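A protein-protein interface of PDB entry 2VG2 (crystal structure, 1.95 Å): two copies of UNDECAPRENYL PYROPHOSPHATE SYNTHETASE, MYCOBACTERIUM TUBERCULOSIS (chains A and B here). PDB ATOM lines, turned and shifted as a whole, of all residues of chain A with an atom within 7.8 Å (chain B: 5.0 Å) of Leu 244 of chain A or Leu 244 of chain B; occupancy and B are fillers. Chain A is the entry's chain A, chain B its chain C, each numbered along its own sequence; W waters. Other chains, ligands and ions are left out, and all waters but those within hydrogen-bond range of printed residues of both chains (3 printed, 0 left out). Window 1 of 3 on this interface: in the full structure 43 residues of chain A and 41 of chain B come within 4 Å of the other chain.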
ATOM      1  N   TYR A 183     -10.467   2.903  -2.153  1.00  0.00           N
ATOM      2  CA  TYR A 183     -10.021   1.548  -2.463  1.00  0.00           C
ATOM      3  C   TYR A 183      -8.549   1.402  -2.106  1.00  0.00           C
ATOM      4  O   TYR A 183      -7.738   2.249  -2.457  1.00  0.00           O
ATOM      5  CB  TYR A 183     -10.213   1.201  -3.956  1.00  0.00           C
ATOM      6  CG  TYR A 183      -9.654  -0.167  -4.298  1.00  0.00           C
ATOM      7  CD1 TYR A 183      -8.288  -0.355  -4.508  1.00  0.00           C
ATOM      8  CD2 TYR A 183     -10.471  -1.290  -4.318  1.00  0.00           C
ATOM      9  CE1 TYR A 183      -7.762  -1.620  -4.740  1.00  0.00           C
ATOM     10  CE2 TYR A 183      -9.960  -2.535  -4.560  1.00  0.00           C
ATOM     11  CZ  TYR A 183      -8.597  -2.702  -4.765  1.00  0.00           C
ATOM     12  OH  TYR A 183      -8.080  -3.966  -5.008  1.00  0.00           O
ATOM     13  N   GLY A 184      -8.209   0.292  -1.441  1.00  0.00           N
ATOM     14  CA  GLY A 184      -6.818  -0.092  -1.227  1.00  0.00           C
ATOM     15  C   GLY A 184      -6.714  -1.601  -1.284  1.00  0.00           C
ATOM     16  O   GLY A 184      -7.435  -2.277  -0.571  1.00  0.00           O
ATOM     17  N   GLY A 185      -5.852  -2.130  -2.161  1.00  0.00           N
ATOM     18  CA  GLY A 185      -5.695  -3.570  -2.335  1.00  0.00           C
ATOM     19  C   GLY A 185      -5.364  -4.345  -1.068  1.00  0.00           C
ATOM     20  O   GLY A 185      -5.967  -5.374  -0.790  1.00  0.00           O
ATOM     21  N   ARG A 186      -4.377  -3.874  -0.313  1.00  0.00           N
ATOM     22  CA  ARG A 186      -4.063  -4.495   0.966  1.00  0.00           C
ATOM     23  C   ARG A 186      -5.250  -4.481   1.909  1.00  0.00           C
ATOM     24  O   ARG A 186      -5.504  -5.464   2.584  1.00  0.00           O
ATOM     25  CB  ARG A 186      -2.901  -3.805   1.645  1.00  0.00           C
ATOM     26  CG  ARG A 186      -1.564  -4.045   0.987  1.00  0.00           C
ATOM     27  CD  ARG A 186      -0.460  -3.550   1.884  1.00  0.00           C
ATOM     28  NE  ARG A 186       0.873  -3.779   1.334  1.00  0.00           N
ATOM     29  CZ  ARG A 186       1.971  -3.247   1.860  1.00  0.00           C
ATOM     30  NH1 ARG A 186       1.884  -2.477   2.940  1.00  0.00           N
ATOM     31  NH2 ARG A 186       3.161  -3.475   1.327  1.00  0.00           N
ATOM     32  N   THR A 187      -5.978  -3.369   1.956  1.00  0.00           N
ATOM     33  CA  THR A 187      -7.138  -3.267   2.850  1.00  0.00           C
ATOM     34  C   THR A 187      -8.228  -4.231   2.414  1.00  0.00           C
ATOM     35  O   THR A 187      -8.834  -4.884   3.234  1.00  0.00           O
ATOM     36  CB  THR A 187      -7.715  -1.824   2.867  1.00  0.00           C
ATOM     37  OG1 THR A 187      -6.687  -0.921   3.248  1.00  0.00           O
ATOM     38  CG2 THR A 187      -8.861  -1.694   3.865  1.00  0.00           C
ATOM     39  N   GLU A 188      -8.473  -4.330   1.110  1.00  0.00           N
ATOM     40  CA  GLU A 188      -9.503  -5.258   0.595  1.00  0.00           C
ATOM     41  C   GLU A 188      -9.165  -6.720   0.943  1.00  0.00           C
ATOM     42  O   GLU A 188     -10.041  -7.504   1.333  1.00  0.00           O
ATOM     43  CB  GLU A 188      -9.643  -5.059  -0.912  1.00  0.00           C
ATOM     44  CG  GLU A 188     -10.422  -6.097  -1.666  1.00  0.00           C
ATOM     45  CD  GLU A 188     -10.580  -5.713  -3.100  1.00  0.00           C
ATOM     46  OE1 GLU A 188      -9.611  -5.893  -3.884  1.00  0.00           O
ATOM     47  OE2 GLU A 188     -11.674  -5.227  -3.451  1.00  0.00           O
ATOM     48  N   ILE A 189      -7.897  -7.074   0.810  1.00  0.00           N
ATOM     49  CA  ILE A 189      -7.418  -8.412   1.198  1.00  0.00           C
ATOM     50  C   ILE A 189      -7.612  -8.611   2.706  1.00  0.00           C
ATOM     51  O   ILE A 189      -8.047  -9.674   3.143  1.00  0.00           O
ATOM     52  CB  ILE A 189      -5.933  -8.613   0.787  1.00  0.00           C
ATOM     53  CG1 ILE A 189      -5.816  -8.782  -0.722  1.00  0.00           C
ATOM     54  CG2 ILE A 189      -5.287  -9.855   1.449  1.00  0.00           C
ATOM     55  CD1 ILE A 189      -4.422  -8.441  -1.239  1.00  0.00           C
ATOM     56  N   LEU A 219     -13.580 -11.560  -1.052  1.00  0.00           N
ATOM     57  CA  LEU A 219     -13.375 -10.166  -1.415  1.00  0.00           C
ATOM     58  C   LEU A 219     -14.730  -9.480  -1.531  1.00  0.00           C
ATOM     59  O   LEU A 219     -15.769 -10.133  -1.712  1.00  0.00           O
ATOM     60  CB  LEU A 219     -12.596 -10.045  -2.725  1.00  0.00           C
ATOM     61  CG  LEU A 219     -11.171 -10.596  -2.769  1.00  0.00           C
ATOM     62  CD1 LEU A 219     -10.656 -10.671  -4.200  1.00  0.00           C
ATOM     63  CD2 LEU A 219     -10.240  -9.762  -1.930  1.00  0.00           C
ATOM     64  N   VAL A 227      -7.605  -8.945 -13.543  1.00  0.00           N
ATOM     65  CA  VAL A 227      -7.277  -7.876 -14.453  1.00  0.00           C
ATOM     66  C   VAL A 227      -6.330  -8.422 -15.518  1.00  0.00           C
ATOM     67  O   VAL A 227      -5.281  -8.989 -15.197  1.00  0.00           O
ATOM     68  CB  VAL A 227      -6.583  -6.714 -13.717  1.00  0.00           C
ATOM     69  CG1 VAL A 227      -6.072  -5.651 -14.717  1.00  0.00           C
ATOM     70  CG2 VAL A 227      -7.530  -6.117 -12.694  1.00  0.00           C
ATOM     71  N   PHE A 230      -3.620  -3.548 -17.254  1.00  0.00           N
ATOM     72  CA  PHE A 230      -3.529  -2.510 -16.233  1.00  0.00           C
ATOM     73  C   PHE A 230      -2.892  -1.296 -16.915  1.00  0.00           C
ATOM     74  O   PHE A 230      -1.727  -1.358 -17.364  1.00  0.00           O
ATOM     75  CB  PHE A 230      -2.655  -3.010 -15.086  1.00  0.00           C
ATOM     76  CG  PHE A 230      -2.686  -2.140 -13.844  1.00  0.00           C
ATOM     77  CD1 PHE A 230      -3.229  -2.629 -12.666  1.00  0.00           C
ATOM     78  CD2 PHE A 230      -2.141  -0.861 -13.849  1.00  0.00           C
ATOM     79  CE1 PHE A 230      -3.243  -1.851 -11.503  1.00  0.00           C
ATOM     80  CE2 PHE A 230      -2.132  -0.060 -12.691  1.00  0.00           C
ATOM     81  CZ  PHE A 230      -2.706  -0.548 -11.521  1.00  0.00           C
ATOM     82  N   SER A 239       1.703   0.412  -9.684  1.00  0.00           N
ATOM     83  CA  SER A 239       0.312  -0.027  -9.594  1.00  0.00           C
ATOM     84  C   SER A 239      -0.395   0.644  -8.401  1.00  0.00           C
ATOM     85  O   SER A 239      -1.618   0.673  -8.342  1.00  0.00           O
ATOM     86  CB  SER A 239       0.235  -1.547  -9.450  1.00  0.00           C
ATOM     87  OG  SER A 239       0.814  -1.979  -8.239  1.00  0.00           O
ATOM     88  N   SER A 240       0.382   1.158  -7.450  1.00  0.00           N
ATOM     89  CA  SER A 240      -0.164   1.937  -6.338  1.00  0.00           C
ATOM     90  C   SER A 240      -1.327   1.242  -5.613  1.00  0.00           C
ATOM     91  O   SER A 240      -2.345   1.864  -5.324  1.00  0.00           O
ATOM     92  CB  SER A 240      -0.595   3.323  -6.816  1.00  0.00           C
ATOM     93  OG  SER A 240       0.521   4.138  -7.157  1.00  0.00           O
ATOM     94  N   ASN A 241      -1.185  -0.059  -5.356  1.00  0.00           N
ATOM     95  CA  ASN A 241      -2.111  -0.774  -4.467  1.00  0.00           C
ATOM     96  C   ASN A 241      -3.486  -0.901  -5.125  1.00  0.00           C
ATOM     97  O   ASN A 241      -4.477  -1.169  -4.455  1.00  0.00           O
ATOM     98  CB  ASN A 241      -2.183  -0.035  -3.109  1.00  0.00           C
ATOM     99  CG  ASN A 241      -2.791  -0.873  -1.971  1.00  0.00           C
ATOM    100  OD1 ASN A 241      -2.697  -2.094  -1.957  1.00  0.00           O
ATOM    101  ND2 ASN A 241      -3.381  -0.181  -0.983  1.00  0.00           N
ATOM    102  N   PHE A 242      -3.556  -0.729  -6.446  1.00  0.00           N
ATOM    103  CA  PHE A 242      -4.826  -0.884  -7.149  1.00  0.00           C
ATOM    104  C   PHE A 242      -5.070  -2.316  -7.640  1.00  0.00           C
ATOM    105  O   PHE A 242      -4.204  -2.911  -8.280  1.00  0.00           O
ATOM    106  CB  PHE A 242      -4.913   0.089  -8.324  1.00  0.00           C
ATOM    107  CG  PHE A 242      -6.288   0.171  -8.950  1.00  0.00           C
ATOM    108  CD1 PHE A 242      -7.427   0.298  -8.163  1.00  0.00           C
ATOM    109  CD2 PHE A 242      -6.443   0.146 -10.336  1.00  0.00           C
ATOM    110  CE1 PHE A 242      -8.679   0.401  -8.722  1.00  0.00           C
ATOM    111  CE2 PHE A 242      -7.719   0.242 -10.906  1.00  0.00           C
ATOM    112  CZ  PHE A 242      -8.822   0.378 -10.095  1.00  0.00           C
ATOM    113  N   MET A 243      -6.264  -2.856  -7.370  1.00  0.00           N
ATOM    114  CA  MET A 243      -6.610  -4.223  -7.762  1.00  0.00           C
ATOM    115  C   MET A 243      -5.494  -5.205  -7.398  1.00  0.00           C
ATOM    116  O   MET A 243      -5.058  -5.998  -8.231  1.00  0.00           O
ATOM    117  CB  MET A 243      -6.879  -4.296  -9.270  1.00  0.00           C
ATOM    118  CG  MET A 243      -8.200  -3.617  -9.700  1.00  0.00           C
ATOM    119  SD  MET A 243      -9.654  -4.513  -9.084  1.00  0.00           S
ATOM    120  CE  MET A 243      -9.699  -5.886 -10.195  1.00  0.00           C
ATOM    121  N   LEU A 244      -5.029  -5.153  -6.153  1.00  0.00           N
ATOM    122  CA  LEU A 244      -3.795  -5.842  -5.806  1.00  0.00           C
ATOM    123  C   LEU A 244      -3.899  -7.358  -6.028  1.00  0.00           C
ATOM    124  O   LEU A 244      -3.066  -7.956  -6.711  1.00  0.00           O
ATOM    125  CB  LEU A 244      -3.392  -5.514  -4.356  1.00  0.00           C
ATOM    126  CG  LEU A 244      -2.068  -6.066  -3.840  1.00  0.00           C
ATOM    127  CD1 LEU A 244      -0.897  -5.523  -4.644  1.00  0.00           C
ATOM    128  CD2 LEU A 244      -1.922  -5.709  -2.363  1.00  0.00           C
ATOM    129  N   TRP A 245      -4.927  -7.979  -5.466  1.00  0.00           N
ATOM    130  CA  TRP A 245      -5.137  -9.402  -5.639  1.00  0.00           C
ATOM    131  C   TRP A 245      -5.421  -9.714  -7.106  1.00  0.00           C
ATOM    132  O   TRP A 245      -4.845 -10.637  -7.681  1.00  0.00           O
ATOM    133  CB  TRP A 245      -6.317  -9.868  -4.801  1.00  0.00           C
ATOM    134  CG  TRP A 245      -6.590 -11.336  -4.876  1.00  0.00           C
ATOM    135  CD1 TRP A 245      -7.460 -11.965  -5.717  1.00  0.00           C
ATOM    136  CD2 TRP A 245      -6.017 -12.368  -4.046  1.00  0.00           C
ATOM    137  NE1 TRP A 245      -7.459 -13.318  -5.471  1.00  0.00           N
ATOM    138  CE2 TRP A 245      -6.588 -13.588  -4.446  1.00  0.00           C
ATOM    139  CE3 TRP A 245      -5.084 -12.370  -2.998  1.00  0.00           C
ATOM    140  CZ2 TRP A 245      -6.246 -14.811  -3.847  1.00  0.00           C
ATOM    141  CZ3 TRP A 245      -4.738 -13.594  -2.402  1.00  0.00           C
ATOM    142  CH2 TRP A 245      -5.324 -14.786  -2.823  1.00  0.00           C
ATOM    143  N   GLN A 246      -6.299  -8.919  -7.706  1.00  0.00           N
ATOM    144  CA  GLN A 246      -6.883  -9.245  -9.012  1.00  0.00           C
ATOM    145  C   GLN A 246      -5.913  -9.048 -10.181  1.00  0.00           C
ATOM    146  O   GLN A 246      -6.075  -9.667 -11.220  1.00  0.00           O
ATOM    147  CB  GLN A 246      -8.111  -8.374  -9.257  1.00  0.00           C
ATOM    148  CG  GLN A 246      -9.211  -8.474  -8.196  1.00  0.00           C
ATOM    149  CD  GLN A 246      -9.061  -7.475  -7.049  1.00  0.00           C
ATOM    150  OE1 GLN A 246      -7.990  -6.896  -6.828  1.00  0.00           O
ATOM    151  NE2 GLN A 246     -10.141  -7.263  -6.322  1.00  0.00           N
ATOM    152  N   ALA A 247      -4.918  -8.185 -10.000  1.00  0.00           N
ATOM    153  CA  ALA A 247      -3.964  -7.840 -11.063  1.00  0.00           C
ATOM    154  C   ALA A 247      -2.618  -8.529 -10.932  1.00  0.00           C
ATOM    155  O   ALA A 247      -1.659  -8.149 -11.607  1.00  0.00           O
ATOM    156  CB  ALA A 247      -3.779  -6.305 -11.102  1.00  0.00           C
ATOM    157  N   ALA A 248      -2.540  -9.564 -10.090  1.00  0.00           N
ATOM    158  CA  ALA A 248      -1.291 -10.316  -9.873  1.00  0.00           C
ATOM    159  C   ALA A 248      -0.596 -10.751 -11.181  1.00  0.00           C
ATOM    160  O   ALA A 248       0.641 -10.775 -11.267  1.00  0.00           O
ATOM    161  CB  ALA A 248      -1.558 -11.542  -8.976  1.00  0.00           C
ATOM    162  N   TYR A 249      -1.404 -11.107 -12.181  1.00  0.00           N
ATOM    163  CA  TYR A 249      -0.926 -11.583 -13.458  1.00  0.00           C
ATOM    164  C   TYR A 249      -1.172 -10.620 -14.627  1.00  0.00           C
ATOM    165  O   TYR A 249      -0.974 -10.996 -15.783  1.00  0.00           O
ATOM    166  CB  TYR A 249      -1.602 -12.924 -13.739  1.00  0.00           C
ATOM    167  CG  TYR A 249      -1.261 -13.978 -12.697  1.00  0.00           C
ATOM    168  CD1 TYR A 249      -0.027 -14.620 -12.706  1.00  0.00           C
ATOM    169  CD2 TYR A 249      -2.179 -14.345 -11.724  1.00  0.00           C
ATOM    170  CE1 TYR A 249       0.284 -15.607 -11.760  1.00  0.00           C
ATOM    171  CE2 TYR A 249      -1.865 -15.326 -10.779  1.00  0.00           C
ATOM    172  CZ  TYR A 249      -0.644 -15.934 -10.803  1.00  0.00           C
ATOM    173  OH  TYR A 249      -0.376 -16.904  -9.860  1.00  0.00           O
ATOM    174  N   TYR A 252       0.947  -4.762 -17.865  1.00  0.00           N
ATOM    175  CA  TYR A 252       0.939  -3.299 -17.680  1.00  0.00           C
ATOM    176  C   TYR A 252       1.276  -2.565 -18.975  1.00  0.00           C
ATOM    177  O   TYR A 252       2.236  -2.924 -19.671  1.00  0.00           O
ATOM    178  CB  TYR A 252       1.966  -2.907 -16.609  1.00  0.00           C
ATOM    179  CG  TYR A 252       1.575  -3.323 -15.223  1.00  0.00           C
ATOM    180  CD1 TYR A 252       0.815  -2.491 -14.433  1.00  0.00           C
ATOM    181  CD2 TYR A 252       1.966  -4.539 -14.696  1.00  0.00           C
ATOM    182  CE1 TYR A 252       0.446  -2.849 -13.165  1.00  0.00           C
ATOM    183  CE2 TYR A 252       1.587  -4.912 -13.390  1.00  0.00           C
ATOM    184  CZ  TYR A 252       0.827  -4.058 -12.644  1.00  0.00           C
ATOM    185  OH  TYR A 252       0.429  -4.368 -11.352  1.00  0.00           O
ATOM    186  N   TYR B 183       7.521 -19.749  -5.065  1.00  0.00           N
ATOM    187  CA  TYR B 183       6.915 -18.553  -4.475  1.00  0.00           C
ATOM    188  C   TYR B 183       5.724 -18.108  -5.326  1.00  0.00           C
ATOM    189  O   TYR B 183       5.794 -18.102  -6.570  1.00  0.00           O
ATOM    190  CB  TYR B 183       7.951 -17.418  -4.357  1.00  0.00           C
ATOM    191  CG  TYR B 183       7.328 -16.147  -3.843  1.00  0.00           C
ATOM    192  CD1 TYR B 183       6.599 -15.322  -4.701  1.00  0.00           C
ATOM    193  CD2 TYR B 183       7.391 -15.813  -2.497  1.00  0.00           C
ATOM    194  CE1 TYR B 183       5.986 -14.186  -4.239  1.00  0.00           C
ATOM    195  CE2 TYR B 183       6.753 -14.661  -2.015  1.00  0.00           C
ATOM    196  CZ  TYR B 183       6.057 -13.859  -2.906  1.00  0.00           C
ATOM    197  OH  TYR B 183       5.415 -12.726  -2.482  1.00  0.00           O
ATOM    198  N   GLY B 185       2.756 -14.790  -4.749  1.00  0.00           N
ATOM    199  CA  GLY B 185       2.240 -13.736  -3.875  1.00  0.00           C
ATOM    200  C   GLY B 185       0.875 -14.042  -3.278  1.00  0.00           C
ATOM    201  O   GLY B 185       0.672 -13.934  -2.072  1.00  0.00           O
ATOM    202  N   ARG B 186      -0.067 -14.435  -4.116  1.00  0.00           N
ATOM    203  CA  ARG B 186      -1.372 -14.868  -3.612  1.00  0.00           C
ATOM    204  C   ARG B 186      -1.258 -16.027  -2.616  1.00  0.00           C
ATOM    205  O   ARG B 186      -1.908 -16.018  -1.586  1.00  0.00           O
ATOM    206  CB  ARG B 186      -2.285 -15.263  -4.759  1.00  0.00           C
ATOM    207  CG  ARG B 186      -2.776 -14.095  -5.616  1.00  0.00           C
ATOM    208  CD  ARG B 186      -3.715 -14.646  -6.673  1.00  0.00           C
ATOM    209  NE  ARG B 186      -4.336 -13.623  -7.510  1.00  0.00           N
ATOM    210  CZ  ARG B 186      -5.070 -13.886  -8.582  1.00  0.00           C
ATOM    211  NH1 ARG B 186      -5.256 -15.140  -8.994  1.00  0.00           N
ATOM    212  NH2 ARG B 186      -5.605 -12.894  -9.275  1.00  0.00           N
ATOM    213  N   ILE B 189       0.079 -14.818   0.827  1.00  0.00           N
ATOM    214  CA  ILE B 189      -1.032 -14.176   1.533  1.00  0.00           C
ATOM    215  C   ILE B 189      -2.031 -15.225   2.043  1.00  0.00           C
ATOM    216  O   ILE B 189      -2.482 -15.155   3.180  1.00  0.00           O
ATOM    217  CB  ILE B 189      -1.754 -13.166   0.612  1.00  0.00           C
ATOM    218  CG1 ILE B 189      -0.866 -11.948   0.361  1.00  0.00           C
ATOM    219  CG2 ILE B 189      -3.089 -12.725   1.208  1.00  0.00           C
ATOM    220  CD1 ILE B 189      -1.230 -11.194  -0.892  1.00  0.00           C
ATOM    221  N   ASN B 241       2.832 -12.009  -9.979  1.00  0.00           N
ATOM    222  CA  ASN B 241       2.514 -12.513  -8.649  1.00  0.00           C
ATOM    223  C   ASN B 241       3.745 -12.502  -7.726  1.00  0.00           C
ATOM    224  O   ASN B 241       3.777 -13.203  -6.717  1.00  0.00           O
ATOM    225  CB  ASN B 241       1.911 -13.924  -8.811  1.00  0.00           C
ATOM    226  CG  ASN B 241       1.145 -14.417  -7.591  1.00  0.00           C
ATOM    227  OD1 ASN B 241       0.575 -13.649  -6.822  1.00  0.00           O
ATOM    228  ND2 ASN B 241       1.097 -15.741  -7.447  1.00  0.00           N
ATOM    229  N   PHE B 242       4.760 -11.702  -8.061  1.00  0.00           N
ATOM    230  CA  PHE B 242       5.994 -11.685  -7.283  1.00  0.00           C
ATOM    231  C   PHE B 242       5.952 -10.585  -6.214  1.00  0.00           C
ATOM    232  O   PHE B 242       5.596  -9.431  -6.503  1.00  0.00           O
ATOM    233  CB  PHE B 242       7.210 -11.530  -8.193  1.00  0.00           C
ATOM    234  CG  PHE B 242       8.521 -11.730  -7.485  1.00  0.00           C
ATOM    235  CD1 PHE B 242       8.706 -12.804  -6.616  1.00  0.00           C
ATOM    236  CD2 PHE B 242       9.573 -10.828  -7.668  1.00  0.00           C
ATOM    237  CE1 PHE B 242       9.933 -12.984  -5.945  1.00  0.00           C
ATOM    238  CE2 PHE B 242      10.785 -11.006  -7.007  1.00  0.00           C
ATOM    239  CZ  PHE B 242      10.963 -12.089  -6.147  1.00  0.00           C
ATOM    240  N   MET B 243       6.292 -10.945  -4.979  1.00  0.00           N
ATOM    241  CA  MET B 243       6.291  -9.993  -3.860  1.00  0.00           C
ATOM    242  C   MET B 243       4.995  -9.185  -3.865  1.00  0.00           C
ATOM    243  O   MET B 243       5.017  -7.951  -3.801  1.00  0.00           O
ATOM    244  CB  MET B 243       7.494  -9.053  -3.988  1.00  0.00           C
ATOM    245  CG  MET B 243       8.840  -9.759  -3.985  1.00  0.00           C
ATOM    246  SD  MET B 243       9.066 -10.942  -2.627  1.00  0.00           S
ATOM    247  CE  MET B 243       8.873  -9.820  -1.301  1.00  0.00           C
ATOM    248  N   LEU B 244       3.863  -9.886  -3.969  1.00  0.00           N
ATOM    249  CA  LEU B 244       2.602  -9.209  -4.252  1.00  0.00           C
ATOM    250  C   LEU B 244       2.218  -8.216  -3.149  1.00  0.00           C
ATOM    251  O   LEU B 244       1.936  -7.045  -3.439  1.00  0.00           O
ATOM    252  CB  LEU B 244       1.487 -10.209  -4.464  1.00  0.00           C
ATOM    253  CG  LEU B 244       0.125  -9.673  -4.881  1.00  0.00           C
ATOM    254  CD1 LEU B 244       0.203  -8.963  -6.231  1.00  0.00           C
ATOM    255  CD2 LEU B 244      -0.913 -10.796  -4.912  1.00  0.00           C
ATOM    256  N   TRP B 245       2.181  -8.688  -1.899  1.00  0.00           N
ATOM    257  CA  TRP B 245       1.902  -7.778  -0.761  1.00  0.00           C
ATOM    258  C   TRP B 245       2.919  -6.645  -0.662  1.00  0.00           C
ATOM    259  O   TRP B 245       2.559  -5.470  -0.492  1.00  0.00           O
ATOM    260  CB  TRP B 245       1.882  -8.577   0.540  1.00  0.00           C
ATOM    261  CG  TRP B 245       1.517  -7.816   1.761  1.00  0.00           C
ATOM    262  CD1 TRP B 245       2.376  -7.212   2.646  1.00  0.00           C
ATOM    263  CD2 TRP B 245       0.192  -7.592   2.274  1.00  0.00           C
ATOM    264  NE1 TRP B 245       1.663  -6.606   3.659  1.00  0.00           N
ATOM    265  CE2 TRP B 245       0.325  -6.831   3.459  1.00  0.00           C
ATOM    266  CE3 TRP B 245      -1.086  -7.956   1.849  1.00  0.00           C
ATOM    267  CZ2 TRP B 245      -0.780  -6.443   4.230  1.00  0.00           C
ATOM    268  CZ3 TRP B 245      -2.182  -7.552   2.608  1.00  0.00           C
ATOM    269  CH2 TRP B 245      -2.015  -6.814   3.789  1.00  0.00           C
ATOM    270  N   GLN B 246       4.182  -7.004  -0.799  1.00  0.00           N
ATOM    271  CA  GLN B 246       5.298  -6.101  -0.482  1.00  0.00           C
ATOM    272  C   GLN B 246       5.515  -5.028  -1.538  1.00  0.00           C
ATOM    273  O   GLN B 246       6.008  -3.954  -1.226  1.00  0.00           O
ATOM    274  CB  GLN B 246       6.590  -6.907  -0.303  1.00  0.00           C
ATOM    275  CG  GLN B 246       6.526  -8.000   0.767  1.00  0.00           C
ATOM    276  CD  GLN B 246       6.029  -9.350   0.253  1.00  0.00           C
ATOM    277  OE1 GLN B 246       5.421  -9.447  -0.811  1.00  0.00           O
ATOM    278  NE2 GLN B 246       6.261 -10.393   1.036  1.00  0.00           N
ATOM    279  N   ALA B 247       5.135  -5.319  -2.784  1.00  0.00           N
ATOM    280  CA  ALA B 247       5.371  -4.394  -3.908  1.00  0.00           C
ATOM    281  C   ALA B 247       4.160  -3.506  -4.266  1.00  0.00           C
ATOM    282  O   ALA B 247       4.134  -2.873  -5.325  1.00  0.00           O
ATOM    283  CB  ALA B 247       5.865  -5.182  -5.144  1.00  0.00           C
ATOM    284  N   ALA B 248       3.174  -3.424  -3.376  1.00  0.00           N
ATOM    285  CA  ALA B 248       1.969  -2.609  -3.649  1.00  0.00           C
ATOM    286  C   ALA B 248       2.267  -1.186  -4.124  1.00  0.00           C
ATOM    287  O   ALA B 248       1.559  -0.662  -4.993  1.00  0.00           O
ATOM    288  CB  ALA B 248       1.042  -2.569  -2.429  1.00  0.00           C
HETATM  289  O   HOH W   1       2.536 -17.434  -9.164  1.00  0.00           O
HETATM  290  O   HOH W   2       3.353  -0.050  -7.405  1.00  0.00           O
HETATM  291  O   HOH W   3       2.363  -3.668  -7.444  1.00  0.00           O
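N of Asn 241 of chain B lies within hydrogen-bond range of O of Ala 248 of chain A (2.8 Å). N of Ser 240 of chain A lies within hydrogen-bond range of O of Ala 248 of chain B (3.3 Å). The side-chain hydroxyl (OH) of Tyr 249 of chain A is in hydrogen-bond range of the side-chain amide nitrogen (ND2) of Asn 241 of chain B (3.1 Å). O of Ala 248 of chain B lies within hydrogen-bond range of N of Asn 241 of chain A, 2.8 Å away. NH2 of Arg 186 of chain B lies within hydrogen-bond range of O of Trp 245 of chain A (2.9 Å). NH2 of Arg 186 of chain A is in hydrogen-bond range of O of Trp 245 of chain B, 2.8 Å away.
The backbone NH of Val 227 of chain A is in hydrogen-bond range of the backbone carbonyl oxygen of Gln 246 of chain A (2.9 Å). The backbone carbonyl oxygen (O) of Asn 241 of chain B lies within hydrogen-bond range of the backbone NH (N) of Gly 185 of chain B (2.7 Å). The backbone NH (N) of Gly 185 of chain A lies within hydrogen-bond range of the backbone carbonyl oxygen (O) of Asn 241 of chain A, 2.8 Å away. OE1 of Gln 246 of chain B sits close to O of Met 243 of chain B (3.4 Å). The backbone carbonyl oxygen of Met 243 of chain A lies close to the side-chain amide oxygen of Gln 246 of chain A (3.4 Å). The side-chain carboxylate (OE1) of Glu 188 of chain A lies within hydrogen-bond range of the side-chain amide nitrogen (NE2) of Gln 246 of chain A (2.8 Å).
Among the printed residues, pairs that only touch across the chains: Arg 186 of chain A with Gln 246 of chain B, Arg 186 of chain A with Ala 248 of chain B, Ile 189 of chain A with Ile 189 of chain B, Ser 239 of chain A with Ala 248 of chain B, Leu 244 of chain A with Leu 244 of chain B, Gln 246 of chain A with Arg 186 of chain B, Ala 248 of chain A with Arg 186 of chain B and Tyr 249 of chain A with Arg 186 of chain B.
Leu 244 of chain A touches just one residue of chain B: Leu 244. Printed residues of chain B within 4 Å of Tyr 249 of chain A: Arg 186 and Asn 241. Of the printed residues of chain A, Ile 189 of chain B touches Ile 189. Of the printed residues of chain A, Gln 246 of chain B touches Arg 186 (3.8 Å). The nearest residue of chain A that does not touch Leu 244 of chain B is Ala 248 of chain A (4.2 Å).
Hydrophobic or aromatic side chains of chain A that line the printed part of chain B: Ile 189, Leu 244, Trp 245, Ala 248 and Tyr 249. Hydrophobic or aromatic side chains of chain B within 4 Å of the printed part of chain A: Ile 189, Leu 244, Trp 245 and Ala 248. Among the printed residues, 14 pairs touch across the chains. Among the printed residues, no Asp or Glu carboxylate lies within 4 Å of a Lys or Arg side-chain nitrogen of the other chain.
Arg 186 of chain A touches Trp 245 of chain B, and with the chains exchanged Trp 245 of chain A touches Arg 186 of chain B. Arg 186 of chain A touches Gln 246 of chain B, and with the chains exchanged Gln 246 of chain A touches Arg 186 of chain B. Arg 186 of chain A touches Ala 248 of chain B, and with the chains exchanged Ala 248 of chain A touches Arg 186 of chain B. Leu 244 of chain A touches its own counterpart, Leu 244 of chain B.
Water W3 lies within hydrogen-bond range of OG of Ser 239 of chain A (2.4 Å) and O of Ala 247 of chain B (2.9 Å). Water W1 lies within hydrogen-bond range of ND2 of Asn 241 of chain B (2.8 Å) and OH of Tyr 249 of chain A (3.0 Å). Water W2 lies within hydrogen-bond range of the backbone NH of Ser 239 of chain A, the backbone carbonyl oxygen of Ala 248 of chain B and the backbone NH of Ser 240 of chain A.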
